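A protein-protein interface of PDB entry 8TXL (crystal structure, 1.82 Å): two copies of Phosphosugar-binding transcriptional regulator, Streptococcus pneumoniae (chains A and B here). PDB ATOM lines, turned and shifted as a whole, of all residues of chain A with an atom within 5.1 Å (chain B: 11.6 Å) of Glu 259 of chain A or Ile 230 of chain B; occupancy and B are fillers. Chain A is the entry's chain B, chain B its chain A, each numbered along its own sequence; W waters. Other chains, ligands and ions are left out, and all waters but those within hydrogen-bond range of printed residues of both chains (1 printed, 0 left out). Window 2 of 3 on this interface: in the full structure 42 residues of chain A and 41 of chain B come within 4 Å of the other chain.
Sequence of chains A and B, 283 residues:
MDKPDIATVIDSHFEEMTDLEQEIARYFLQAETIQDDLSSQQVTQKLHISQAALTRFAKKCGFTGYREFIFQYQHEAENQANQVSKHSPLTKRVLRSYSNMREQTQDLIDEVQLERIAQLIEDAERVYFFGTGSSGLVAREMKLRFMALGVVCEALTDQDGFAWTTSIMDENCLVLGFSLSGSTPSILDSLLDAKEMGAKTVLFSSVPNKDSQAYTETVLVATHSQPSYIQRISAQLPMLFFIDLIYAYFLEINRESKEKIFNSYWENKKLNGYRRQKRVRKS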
ATOM      1  N   ARG A 145      22.709   4.111  11.857  1.00  0.00           N
ATOM      2  CA  ARG A 145      22.874   4.851  10.610  1.00  0.00           C
ATOM      3  C   ARG A 145      22.595   6.338  10.800  1.00  0.00           C
ATOM      4  O   ARG A 145      23.322   7.183  10.269  1.00  0.00           O
ATOM      5  CB  ARG A 145      21.955   4.255   9.551  1.00  0.00           C
ATOM      6  CG  ARG A 145      22.051   2.733   9.501  1.00  0.00           C
ATOM      7  CD  ARG A 145      22.063   2.306   8.069  1.00  0.00           C
ATOM      8  NE  ARG A 145      23.176   2.932   7.352  1.00  0.00           N
ATOM      9  CZ  ARG A 145      23.277   2.955   6.032  1.00  0.00           C
ATOM     10  NH1 ARG A 145      22.322   2.444   5.262  1.00  0.00           N
ATOM     11  NH2 ARG A 145      24.325   3.565   5.464  1.00  0.00           N
ATOM     12  N   LEU A 149      25.308  10.263  11.373  1.00  0.00           N
ATOM     13  CA  LEU A 149      25.135  11.548  10.713  1.00  0.00           C
ATOM     14  C   LEU A 149      24.856  12.677  11.695  1.00  0.00           C
ATOM     15  O   LEU A 149      24.602  13.804  11.261  1.00  0.00           O
ATOM     16  CB  LEU A 149      23.996  11.482   9.678  1.00  0.00           C
ATOM     17  CG  LEU A 149      24.097  10.387   8.615  1.00  0.00           C
ATOM     18  CD1 LEU A 149      22.965  10.439   7.614  1.00  0.00           C
ATOM     19  CD2 LEU A 149      25.453  10.452   7.888  1.00  0.00           C
ATOM     20  N   TYR A 247      16.569   7.175   4.772  1.00  0.00           N
ATOM     21  CA  TYR A 247      17.961   7.524   5.034  1.00  0.00           C
ATOM     22  C   TYR A 247      18.574   8.223   3.825  1.00  0.00           C
ATOM     23  O   TYR A 247      19.279   9.232   3.967  1.00  0.00           O
ATOM     24  CB  TYR A 247      18.773   6.273   5.370  1.00  0.00           C
ATOM     25  CG  TYR A 247      20.245   6.534   5.466  1.00  0.00           C
ATOM     26  CD1 TYR A 247      20.803   7.005   6.645  1.00  0.00           C
ATOM     27  CD2 TYR A 247      21.075   6.305   4.382  1.00  0.00           C
ATOM     28  CE1 TYR A 247      22.164   7.219   6.745  1.00  0.00           C
ATOM     29  CE2 TYR A 247      22.449   6.541   4.463  1.00  0.00           C
ATOM     30  CZ  TYR A 247      22.975   6.995   5.658  1.00  0.00           C
ATOM     31  OH  TYR A 247      24.316   7.244   5.782  1.00  0.00           O
ATOM     32  N   LEU A 251      20.062  12.031   4.081  1.00  0.00           N
ATOM     33  CA  LEU A 251      21.472  12.329   3.876  1.00  0.00           C
ATOM     34  C   LEU A 251      21.648  13.510   2.937  1.00  0.00           C
ATOM     35  O   LEU A 251      22.641  14.239   3.038  1.00  0.00           O
ATOM     36  CB  LEU A 251      22.167  11.088   3.315  1.00  0.00           C
ATOM     37  CG  LEU A 251      23.602  11.226   2.804  1.00  0.00           C
ATOM     38  CD1 LEU A 251      24.499  11.725   3.875  1.00  0.00           C
ATOM     39  CD2 LEU A 251      24.146   9.914   2.247  1.00  0.00           C
ATOM     40  N   ARG A 255      23.830  17.824   3.124  1.00  0.00           N
ATOM     41  CA  ARG A 255      24.765  16.719   2.915  1.00  0.00           C
ATOM     42  C   ARG A 255      26.151  17.013   3.469  1.00  0.00           C
ATOM     43  O   ARG A 255      26.750  16.167   4.142  1.00  0.00           O
ATOM     44  CB  ARG A 255      24.829  16.423   1.418  1.00  0.00           C
ATOM     45  CG  ARG A 255      25.820  15.401   0.989  1.00  0.00           C
ATOM     46  CD  ARG A 255      25.565  14.066   1.582  1.00  0.00           C
ATOM     47  NE  ARG A 255      26.641  13.167   1.196  1.00  0.00           N
ATOM     48  CZ  ARG A 255      26.508  12.262   0.249  1.00  0.00           C
ATOM     49  NH1 ARG A 255      25.379  12.155  -0.432  1.00  0.00           N
ATOM     50  NH2 ARG A 255      27.527  11.437  -0.015  1.00  0.00           N
ATOM     51  N   GLU A 256      26.715  18.177   3.155  1.00  0.00           N
ATOM     52  CA  GLU A 256      28.101  18.392   3.545  1.00  0.00           C
ATOM     53  C   GLU A 256      28.257  18.425   5.064  1.00  0.00           C
ATOM     54  O   GLU A 256      29.193  17.834   5.602  1.00  0.00           O
ATOM     55  CB  GLU A 256      28.643  19.656   2.875  1.00  0.00           C
ATOM     56  CG  GLU A 256      29.100  19.352   1.417  1.00  0.00           C
ATOM     57  CD  GLU A 256      30.573  18.940   1.332  1.00  0.00           C
ATOM     58  OE1 GLU A 256      30.969  17.837   1.821  1.00  0.00           O
ATOM     59  OE2 GLU A 256      31.353  19.744   0.807  1.00  0.00           O
ATOM     60  N   SER A 257      27.344  19.070   5.785  1.00  0.00           N
ATOM     61  CA  SER A 257      27.444  19.057   7.242  1.00  0.00           C
ATOM     62  C   SER A 257      27.364  17.633   7.778  1.00  0.00           C
ATOM     63  O   SER A 257      28.084  17.274   8.722  1.00  0.00           O
ATOM     64  CB  SER A 257      26.354  19.928   7.863  1.00  0.00           C
ATOM     65  OG  SER A 257      25.131  19.215   7.942  1.00  0.00           O
ATOM     66  N   LYS A 258      26.505  16.798   7.176  1.00  0.00           N
ATOM     67  CA  LYS A 258      26.373  15.417   7.641  1.00  0.00           C
ATOM     68  C   LYS A 258      27.581  14.577   7.259  1.00  0.00           C
ATOM     69  O   LYS A 258      27.971  13.685   8.012  1.00  0.00           O
ATOM     70  CB  LYS A 258      25.078  14.777   7.102  1.00  0.00           C
ATOM     71  CG  LYS A 258      23.864  15.262   7.900  1.00  0.00           C
ATOM     72  CD  LYS A 258      22.544  15.088   7.221  1.00  0.00           C
ATOM     73  CE  LYS A 258      21.449  15.803   8.030  1.00  0.00           C
ATOM     74  NZ  LYS A 258      20.106  15.726   7.400  1.00  0.00           N
ATOM     75  N   GLU A 259      28.193  14.835   6.111  1.00  0.00           N
ATOM     76  CA  GLU A 259      29.385  14.076   5.749  1.00  0.00           C
ATOM     77  C   GLU A 259      30.561  14.446   6.654  1.00  0.00           C
ATOM     78  O   GLU A 259      31.378  13.584   7.006  1.00  0.00           O
ATOM     79  CB  GLU A 259      29.708  14.297   4.261  1.00  0.00           C
ATOM     80  CG  GLU A 259      30.679  13.275   3.726  1.00  0.00           C
ATOM     81  CD  GLU A 259      30.314  12.742   2.364  1.00  0.00           C
ATOM     82  OE1 GLU A 259      29.404  13.288   1.703  1.00  0.00           O
ATOM     83  OE2 GLU A 259      30.927  11.736   1.958  1.00  0.00           O
ATOM     84  N   LYS A 260      30.637  15.718   7.061  1.00  0.00           N
ATOM     85  CA  LYS A 260      31.649  16.165   8.011  1.00  0.00           C
ATOM     86  C   LYS A 260      31.547  15.354   9.295  1.00  0.00           C
ATOM     87  O   LYS A 260      32.555  14.891   9.854  1.00  0.00           O
ATOM     88  CB  LYS A 260      31.430  17.654   8.266  1.00  0.00           C
ATOM     89  CG  LYS A 260      32.592  18.588   8.032  1.00  0.00           C
ATOM     90  CD  LYS A 260      32.751  18.859   6.526  1.00  0.00           C
ATOM     91  CE  LYS A 260      33.252  20.261   6.230  1.00  0.00           C
ATOM     92  NZ  LYS A 260      33.465  20.556   4.786  1.00  0.00           N
ATOM     93  N   ILE A 261      30.311  15.140   9.742  1.00  0.00           N
ATOM     94  CA  ILE A 261      30.068  14.460  11.012  1.00  0.00           C
ATOM     95  C   ILE A 261      30.439  12.987  10.902  1.00  0.00           C
ATOM     96  O   ILE A 261      31.127  12.426  11.768  1.00  0.00           O
ATOM     97  CB  ILE A 261      28.593  14.650  11.423  1.00  0.00           C
ATOM     98  CG1 ILE A 261      28.344  16.140  11.686  1.00  0.00           C
ATOM     99  CG2 ILE A 261      28.229  13.776  12.636  1.00  0.00           C
ATOM    100  CD1 ILE A 261      26.925  16.502  12.043  1.00  0.00           C
ATOM    101  N   PHE A 262      29.971  12.335   9.838  1.00  0.00           N
ATOM    102  CA  PHE A 262      30.371  10.971   9.514  1.00  0.00           C
ATOM    103  C   PHE A 262      31.889  10.847   9.387  1.00  0.00           C
ATOM    104  O   PHE A 262      32.479   9.887   9.876  1.00  0.00           O
ATOM    105  CB  PHE A 262      29.644  10.589   8.231  1.00  0.00           C
ATOM    106  CG  PHE A 262      29.768   9.159   7.794  1.00  0.00           C
ATOM    107  CD1 PHE A 262      30.742   8.766   6.885  1.00  0.00           C
ATOM    108  CD2 PHE A 262      28.811   8.239   8.178  1.00  0.00           C
ATOM    109  CE1 PHE A 262      30.799   7.454   6.433  1.00  0.00           C
ATOM    110  CE2 PHE A 262      28.869   6.933   7.758  1.00  0.00           C
ATOM    111  CZ  PHE A 262      29.846   6.535   6.868  1.00  0.00           C
ATOM    112  N   ASN A 263      32.551  11.793   8.729  1.00  0.00           N
ATOM    113  CA  ASN A 263      34.004  11.666   8.619  1.00  0.00           C
ATOM    114  C   ASN A 263      34.705  11.968   9.936  1.00  0.00           C
ATOM    115  O   ASN A 263      35.706  11.329  10.275  1.00  0.00           O
ATOM    116  CB  ASN A 263      34.506  12.569   7.501  1.00  0.00           C
ATOM    117  CG  ASN A 263      34.217  12.006   6.137  1.00  0.00           C
ATOM    118  OD1 ASN A 263      33.991  10.809   5.977  1.00  0.00           O
ATOM    119  ND2 ASN A 263      34.259  12.870   5.129  1.00  0.00           N
ATOM    120  N   SER A 264      34.206  12.939  10.688  1.00  0.00           N
ATOM    121  CA  SER A 264      34.743  13.192  12.015  1.00  0.00           C
ATOM    122  C   SER A 264      34.660  11.945  12.919  1.00  0.00           C
ATOM    123  O   SER A 264      35.600  11.669  13.681  1.00  0.00           O
ATOM    124  CB  SER A 264      34.017  14.378  12.638  1.00  0.00           C
ATOM    125  OG  SER A 264      34.898  15.095  13.481  1.00  0.00           O
ATOM    126  N   LEU B  90      17.289   9.580  -6.827  1.00  0.00           N
ATOM    127  CA  LEU B  90      17.616   9.082  -5.495  1.00  0.00           C
ATOM    128  C   LEU B  90      16.899   7.763  -5.213  1.00  0.00           C
ATOM    129  O   LEU B  90      17.523   6.760  -4.817  1.00  0.00           O
ATOM    130  CB  LEU B  90      17.225  10.128  -4.443  1.00  0.00           C
ATOM    131  CG  LEU B  90      18.312  10.658  -3.513  1.00  0.00           C
ATOM    132  CD1 LEU B  90      17.775  11.523  -2.365  1.00  0.00           C
ATOM    133  CD2 LEU B  90      19.180   9.512  -2.980  1.00  0.00           C
ATOM    134  N   ARG B  93      18.288   4.901  -7.247  1.00  0.00           N
ATOM    135  CA  ARG B  93      19.567   4.436  -6.713  1.00  0.00           C
ATOM    136  C   ARG B  93      19.352   3.414  -5.599  1.00  0.00           C
ATOM    137  O   ARG B  93      20.006   2.365  -5.568  1.00  0.00           O
ATOM    138  CB  ARG B  93      20.370   5.609  -6.172  1.00  0.00           C
ATOM    139  CG  ARG B  93      21.840   5.273  -5.834  1.00  0.00           C
ATOM    140  CD  ARG B  93      22.487   6.383  -4.993  1.00  0.00           C
ATOM    141  NE  ARG B  93      22.103   6.243  -3.588  1.00  0.00           N
ATOM    142  CZ  ARG B  93      22.124   7.213  -2.681  1.00  0.00           C
ATOM    143  NH1 ARG B  93      22.478   8.450  -2.992  1.00  0.00           N
ATOM    144  NH2 ARG B  93      21.775   6.934  -1.424  1.00  0.00           N
ATOM    145  N   VAL B  94      18.403   3.691  -4.702  1.00  0.00           N
ATOM    146  CA  VAL B  94      18.175   2.798  -3.559  1.00  0.00           C
ATOM    147  C   VAL B  94      17.609   1.470  -4.032  1.00  0.00           C
ATOM    148  O   VAL B  94      18.074   0.394  -3.627  1.00  0.00           O
ATOM    149  CB  VAL B  94      17.244   3.464  -2.525  1.00  0.00           C
ATOM    150  CG1 VAL B  94      16.845   2.443  -1.476  1.00  0.00           C
ATOM    151  CG2 VAL B  94      17.904   4.653  -1.885  1.00  0.00           C
ATOM    152  N   SER B  97      20.233  -0.578  -5.630  1.00  0.00           N
ATOM    153  CA  SER B  97      21.095  -1.224  -4.626  1.00  0.00           C
ATOM    154  C   SER B  97      20.494  -2.538  -4.150  1.00  0.00           C
ATOM    155  O   SER B  97      21.192  -3.549  -4.049  1.00  0.00           O
ATOM    156  CB  SER B  97      21.341  -0.272  -3.469  1.00  0.00           C
ATOM    157  OG  SER B  97      22.257   0.728  -3.830  1.00  0.00           O
ATOM    158  N   HIS B 224      28.283  -4.565  -1.313  1.00  0.00           N
ATOM    159  CA  HIS B 224      27.357  -3.484  -1.635  1.00  0.00           C
ATOM    160  C   HIS B 224      27.683  -2.848  -2.985  1.00  0.00           C
ATOM    161  O   HIS B 224      28.835  -2.720  -3.378  1.00  0.00           O
ATOM    162  CB  HIS B 224      27.408  -2.411  -0.558  1.00  0.00           C
ATOM    163  CG  HIS B 224      26.709  -2.804   0.703  1.00  0.00           C
ATOM    164  ND1 HIS B 224      27.268  -3.661   1.622  1.00  0.00           N
ATOM    165  CD2 HIS B 224      25.494  -2.460   1.188  1.00  0.00           C
ATOM    166  CE1 HIS B 224      26.420  -3.837   2.628  1.00  0.00           C
ATOM    167  NE2 HIS B 224      25.338  -3.121   2.391  1.00  0.00           N
ATOM    168  N   SER B 225      26.634  -2.446  -3.707  1.00  0.00           N
ATOM    169  CA  SER B 225      26.831  -1.856  -5.029  1.00  0.00           C
ATOM    170  C   SER B 225      27.396  -0.445  -4.926  1.00  0.00           C
ATOM    171  O   SER B 225      28.128  -0.006  -5.816  1.00  0.00           O
ATOM    172  CB  SER B 225      25.522  -1.844  -5.801  1.00  0.00           C
ATOM    173  OG  SER B 225      24.831  -0.656  -5.455  1.00  0.00           O
ATOM    174  N   GLN B 226      27.097   0.266  -3.847  1.00  0.00           N
ATOM    175  CA  GLN B 226      27.585   1.634  -3.672  1.00  0.00           C
ATOM    176  C   GLN B 226      29.016   1.631  -3.130  1.00  0.00           C
ATOM    177  O   GLN B 226      29.288   0.990  -2.105  1.00  0.00           O
ATOM    178  CB  GLN B 226      26.665   2.409  -2.716  1.00  0.00           C
ATOM    179  CG  GLN B 226      25.313   2.827  -3.339  1.00  0.00           C
ATOM    180  CD  GLN B 226      25.471   3.976  -4.311  1.00  0.00           C
ATOM    181  OE1 GLN B 226      26.099   4.990  -3.990  1.00  0.00           O
ATOM    182  NE2 GLN B 226      24.894   3.841  -5.499  1.00  0.00           N
ATOM    183  N   PRO B 227      29.946   2.346  -3.767  1.00  0.00           N
ATOM    184  CA  PRO B 227      31.328   2.343  -3.253  1.00  0.00           C
ATOM    185  C   PRO B 227      31.467   2.967  -1.879  1.00  0.00           C
ATOM    186  O   PRO B 227      32.076   2.361  -0.982  1.00  0.00           O
ATOM    187  CB  PRO B 227      32.096   3.145  -4.319  1.00  0.00           C
ATOM    188  CG  PRO B 227      31.256   3.103  -5.527  1.00  0.00           C
ATOM    189  CD  PRO B 227      29.837   3.048  -5.055  1.00  0.00           C
ATOM    190  N   SER B 228      30.928   4.170  -1.686  1.00  0.00           N
ATOM    191  CA  SER B 228      31.141   4.901  -0.447  1.00  0.00           C
ATOM    192  C   SER B 228      30.255   4.357   0.661  1.00  0.00           C
ATOM    193  O   SER B 228      29.096   3.978   0.441  1.00  0.00           O
ATOM    194  CB  SER B 228      30.871   6.391  -0.636  1.00  0.00           C
ATOM    195  OG  SER B 228      29.485   6.651  -0.701  1.00  0.00           O
ATOM    196  N   TYR B 229      30.823   4.321   1.859  1.00  0.00           N
ATOM    197  CA  TYR B 229      30.122   3.770   3.005  1.00  0.00           C
ATOM    198  C   TYR B 229      28.829   4.521   3.285  1.00  0.00           C
ATOM    199  O   TYR B 229      27.789   3.901   3.537  1.00  0.00           O
ATOM    200  CB  TYR B 229      31.066   3.807   4.199  1.00  0.00           C
ATOM    201  CG  TYR B 229      31.712   2.486   4.484  1.00  0.00           C
ATOM    202  CD1 TYR B 229      30.934   1.353   4.635  1.00  0.00           C
ATOM    203  CD2 TYR B 229      33.085   2.368   4.644  1.00  0.00           C
ATOM    204  CE1 TYR B 229      31.503   0.132   4.896  1.00  0.00           C
ATOM    205  CE2 TYR B 229      33.668   1.147   4.925  1.00  0.00           C
ATOM    206  CZ  TYR B 229      32.862   0.029   5.059  1.00  0.00           C
ATOM    207  OH  TYR B 229      33.381  -1.220   5.325  1.00  0.00           O
ATOM    208  N   ILE B 230      28.867   5.853   3.206  1.00  0.00           N
ATOM    209  CA  ILE B 230      27.775   6.698   3.697  1.00  0.00           C
ATOM    210  C   ILE B 230      26.520   6.554   2.860  1.00  0.00           C
ATOM    211  O   ILE B 230      25.423   6.867   3.336  1.00  0.00           O
ATOM    212  CB  ILE B 230      28.300   8.147   3.764  1.00  0.00           C
ATOM    213  CG1 ILE B 230      27.423   9.047   4.600  1.00  0.00           C
ATOM    214  CG2 ILE B 230      28.485   8.700   2.337  1.00  0.00           C
ATOM    215  CD1 ILE B 230      28.090  10.393   4.889  1.00  0.00           C
ATOM    216  N   GLN B 231      26.637   6.023   1.655  1.00  0.00           N
ATOM    217  CA  GLN B 231      25.501   5.867   0.764  1.00  0.00           C
ATOM    218  C   GLN B 231      25.011   4.435   0.644  1.00  0.00           C
ATOM    219  O   GLN B 231      24.074   4.181  -0.132  1.00  0.00           O
ATOM    220  CB  GLN B 231      25.832   6.393  -0.658  1.00  0.00           C
ATOM    221  CG  GLN B 231      25.962   7.882  -0.693  1.00  0.00           C
ATOM    222  CD  GLN B 231      25.999   8.481  -2.094  1.00  0.00           C
ATOM    223  OE1 GLN B 231      25.924   9.699  -2.226  1.00  0.00           O
ATOM    224  NE2 GLN B 231      26.059   7.641  -3.135  1.00  0.00           N
ATOM    225  N   ARG B 232      25.611   3.497   1.370  1.00  0.00           N
ATOM    226  CA  ARG B 232      25.202   2.116   1.225  1.00  0.00           C
ATOM    227  C   ARG B 232      23.836   1.889   1.866  1.00  0.00           C
ATOM    228  O   ARG B 232      23.468   2.564   2.835  1.00  0.00           O
ATOM    229  CB  ARG B 232      26.232   1.206   1.879  1.00  0.00           C
ATOM    230  CG  ARG B 232      27.493   1.075   1.071  1.00  0.00           C
ATOM    231  CD  ARG B 232      28.516   0.267   1.824  1.00  0.00           C
ATOM    232  NE  ARG B 232      29.756   0.205   1.062  1.00  0.00           N
ATOM    233  CZ  ARG B 232      30.795  -0.539   1.400  1.00  0.00           C
ATOM    234  NH1 ARG B 232      30.760  -1.326   2.465  1.00  0.00           N
ATOM    235  NH2 ARG B 232      31.898  -0.483   0.660  1.00  0.00           N
ATOM    236  N   ILE B 233      23.114   0.898   1.344  1.00  0.00           N
ATOM    237  CA  ILE B 233      21.899   0.424   2.010  1.00  0.00           C
ATOM    238  C   ILE B 233      22.271  -0.476   3.187  1.00  0.00           C
ATOM    239  O   ILE B 233      23.455  -0.619   3.514  1.00  0.00           O
ATOM    240  CB  ILE B 233      20.991  -0.318   1.031  1.00  0.00           C
ATOM    241  CG1 ILE B 233      21.697  -1.509   0.424  1.00  0.00           C
ATOM    242  CG2 ILE B 233      20.536   0.682  -0.051  1.00  0.00           C
ATOM    243  CD1 ILE B 233      20.739  -2.512  -0.239  1.00  0.00           C
ATOM    244  N   SER B 234      21.264  -1.103   3.806  1.00  0.00           N
ATOM    245  CA  SER B 234      21.466  -1.794   5.073  1.00  0.00           C
ATOM    246  C   SER B 234      22.645  -2.753   5.002  1.00  0.00           C
ATOM    247  O   SER B 234      22.784  -3.530   4.052  1.00  0.00           O
ATOM    248  CB  SER B 234      20.197  -2.576   5.441  1.00  0.00           C
ATOM    249  OG  SER B 234      20.465  -3.462   6.518  1.00  0.00           O
ATOM    250  N   ALA B 235      23.502  -2.678   6.000  1.00  0.00           N
ATOM    251  CA  ALA B 235      24.617  -3.612   6.103  1.00  0.00           C
ATOM    252  C   ALA B 235      24.163  -5.023   6.450  1.00  0.00           C
ATOM    253  O   ALA B 235      24.923  -5.964   6.242  1.00  0.00           O
ATOM    254  CB  ALA B 235      25.613  -3.149   7.177  1.00  0.00           C
HETATM  255  O   HOH W   1      29.073   9.586  -1.210  1.00  0.00           O
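NE2 of His 224 of chain B is in hydrogen-bond range of O of Ser 234 of chain B. O of Pro 227 of chain B sits at hydrogen-bond distance from NH2 of Arg 232 of chain B, at 3.3 Å. The backbone carbonyl oxygen (O) of Gln 226 of chain B is in hydrogen-bond range of the guanidinium group (NE) of Arg 232 of chain B (3.3 Å). NE2 of His 224 of chain B sits at hydrogen-bond distance from O of Ile 233 of chain B, 3.3 Å away. The guanidinium group (NE) of Arg 255 of chain A lies within salt-bridge range of the side-chain carboxylate (OE1) of Glu 259 of chain A (2.8 Å). The side-chain amide nitrogen (NE2) of Gln 231 of chain B sits at hydrogen-bond distance from the side-chain amide oxygen (OE1) of Gln 226 of chain B (2.8 Å).
Of the printed residues of chain B, Arg 145 of chain A touches Tyr 229 (3.98 Å), Arg 232 (2.7 Å), Ile 233 (3.6 Å) and Ser 234 (3.98 Å). Of the printed residues of chain B, Tyr 247 of chain A touches Ile 230 (2.7 Å). Glu 256 of chain A touches none of the printed residues of chain B. No residue of chain B comes within 4 Å of Ser 257 of chain A. Lys 258 of chain A touches none of the printed residues of chain B. Of chain B, only Ile 230 comes within 4 Å of Glu 259 of chain A. No residue of chain B comes within 4 Å of Lys 260 of chain A. No residue of chain B comes within 4 Å of Ile 261 of chain A. Asn 263 of chain A touches none of the printed residues of chain B. Ser 97 of chain B touches none of the printed residues of chain A. Printed residues of chain A within 4 Å of Tyr 229 of chain B: Arg 145 (3.98 Å). Printed residues of chain A within 4 Å of Ile 230 of chain B: Leu 149 (3.99 Å), Tyr 247 (2.7 Å), Leu 251 (3.5 Å), Arg 255 (3.7 Å), Glu 259 (3.9 Å) and Phe 262 (3.6 Å). Of the printed residues of chain A, Arg 232 of chain B touches Arg 145 (2.7 Å). The nearest printed residue of chain B that does not touch Leu 251 of chain A is Gln 231 of chain B (4.01 Å).
Among the printed residues, merely in contact across the chains: Arg 145 of chain A with Tyr 229 of chain B, Arg 145 of chain A with Ile 233 of chain B, Arg 145 of chain A with Ser 234 of chain B, Leu 149 of chain A with Ile 230 of chain B, Leu 251 of chain A with Ile 230 of chain B, Arg 255 of chain A with Ile 230 of chain B, Glu 259 of chain A with Ile 230 of chain B and Phe 262 of chain A with Ile 230 of chain B.
No position is printed for both chains. Of the 11 pairs that touch across the chains among the printed residues, none has its exchanged pair printed and touching as well.
Water W1 lies within hydrogen-bond range of the guanidinium group (NH2) of Arg 255 of chain A, the side-chain hydroxyl (OG) of Ser 228 of chain B and the side-chain amide oxygen (OE1) of Gln 231 of chain B.
NH1 of Arg 145 of chain A is in hydrogen-bond range of O of Arg 232 of chain B, at 2.7 Å. The backbone carbonyl oxygen (O) of Ile 230 of chain B lies within hydrogen-bond range of the side-chain hydroxyl (OH) of Tyr 247 of chain A, 2.7 Å away. NH1 of Arg 255 of chain A sits at hydrogen-bond distance from OE1 of Gln 231 of chain B, at 3.1 Å.
Of the 14 printed residues of chain A, 7 touch a printed residue of chain B. Hydrophobic or aromatic side chains of chain A that line the printed part of chain B: Leu 149, Tyr 247, Leu 251 and Phe 262. Printed residues of chain B that touch a printed residue of chain A: Tyr 229, Ile 230, Gln 231, Arg 232, Ile 233 and Ser 234. Hydrophobic or aromatic side chains of chain B within 4 Å of the printed part of chain A: Ile 230. Among the printed residues, 11 pairs touch across the chains.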
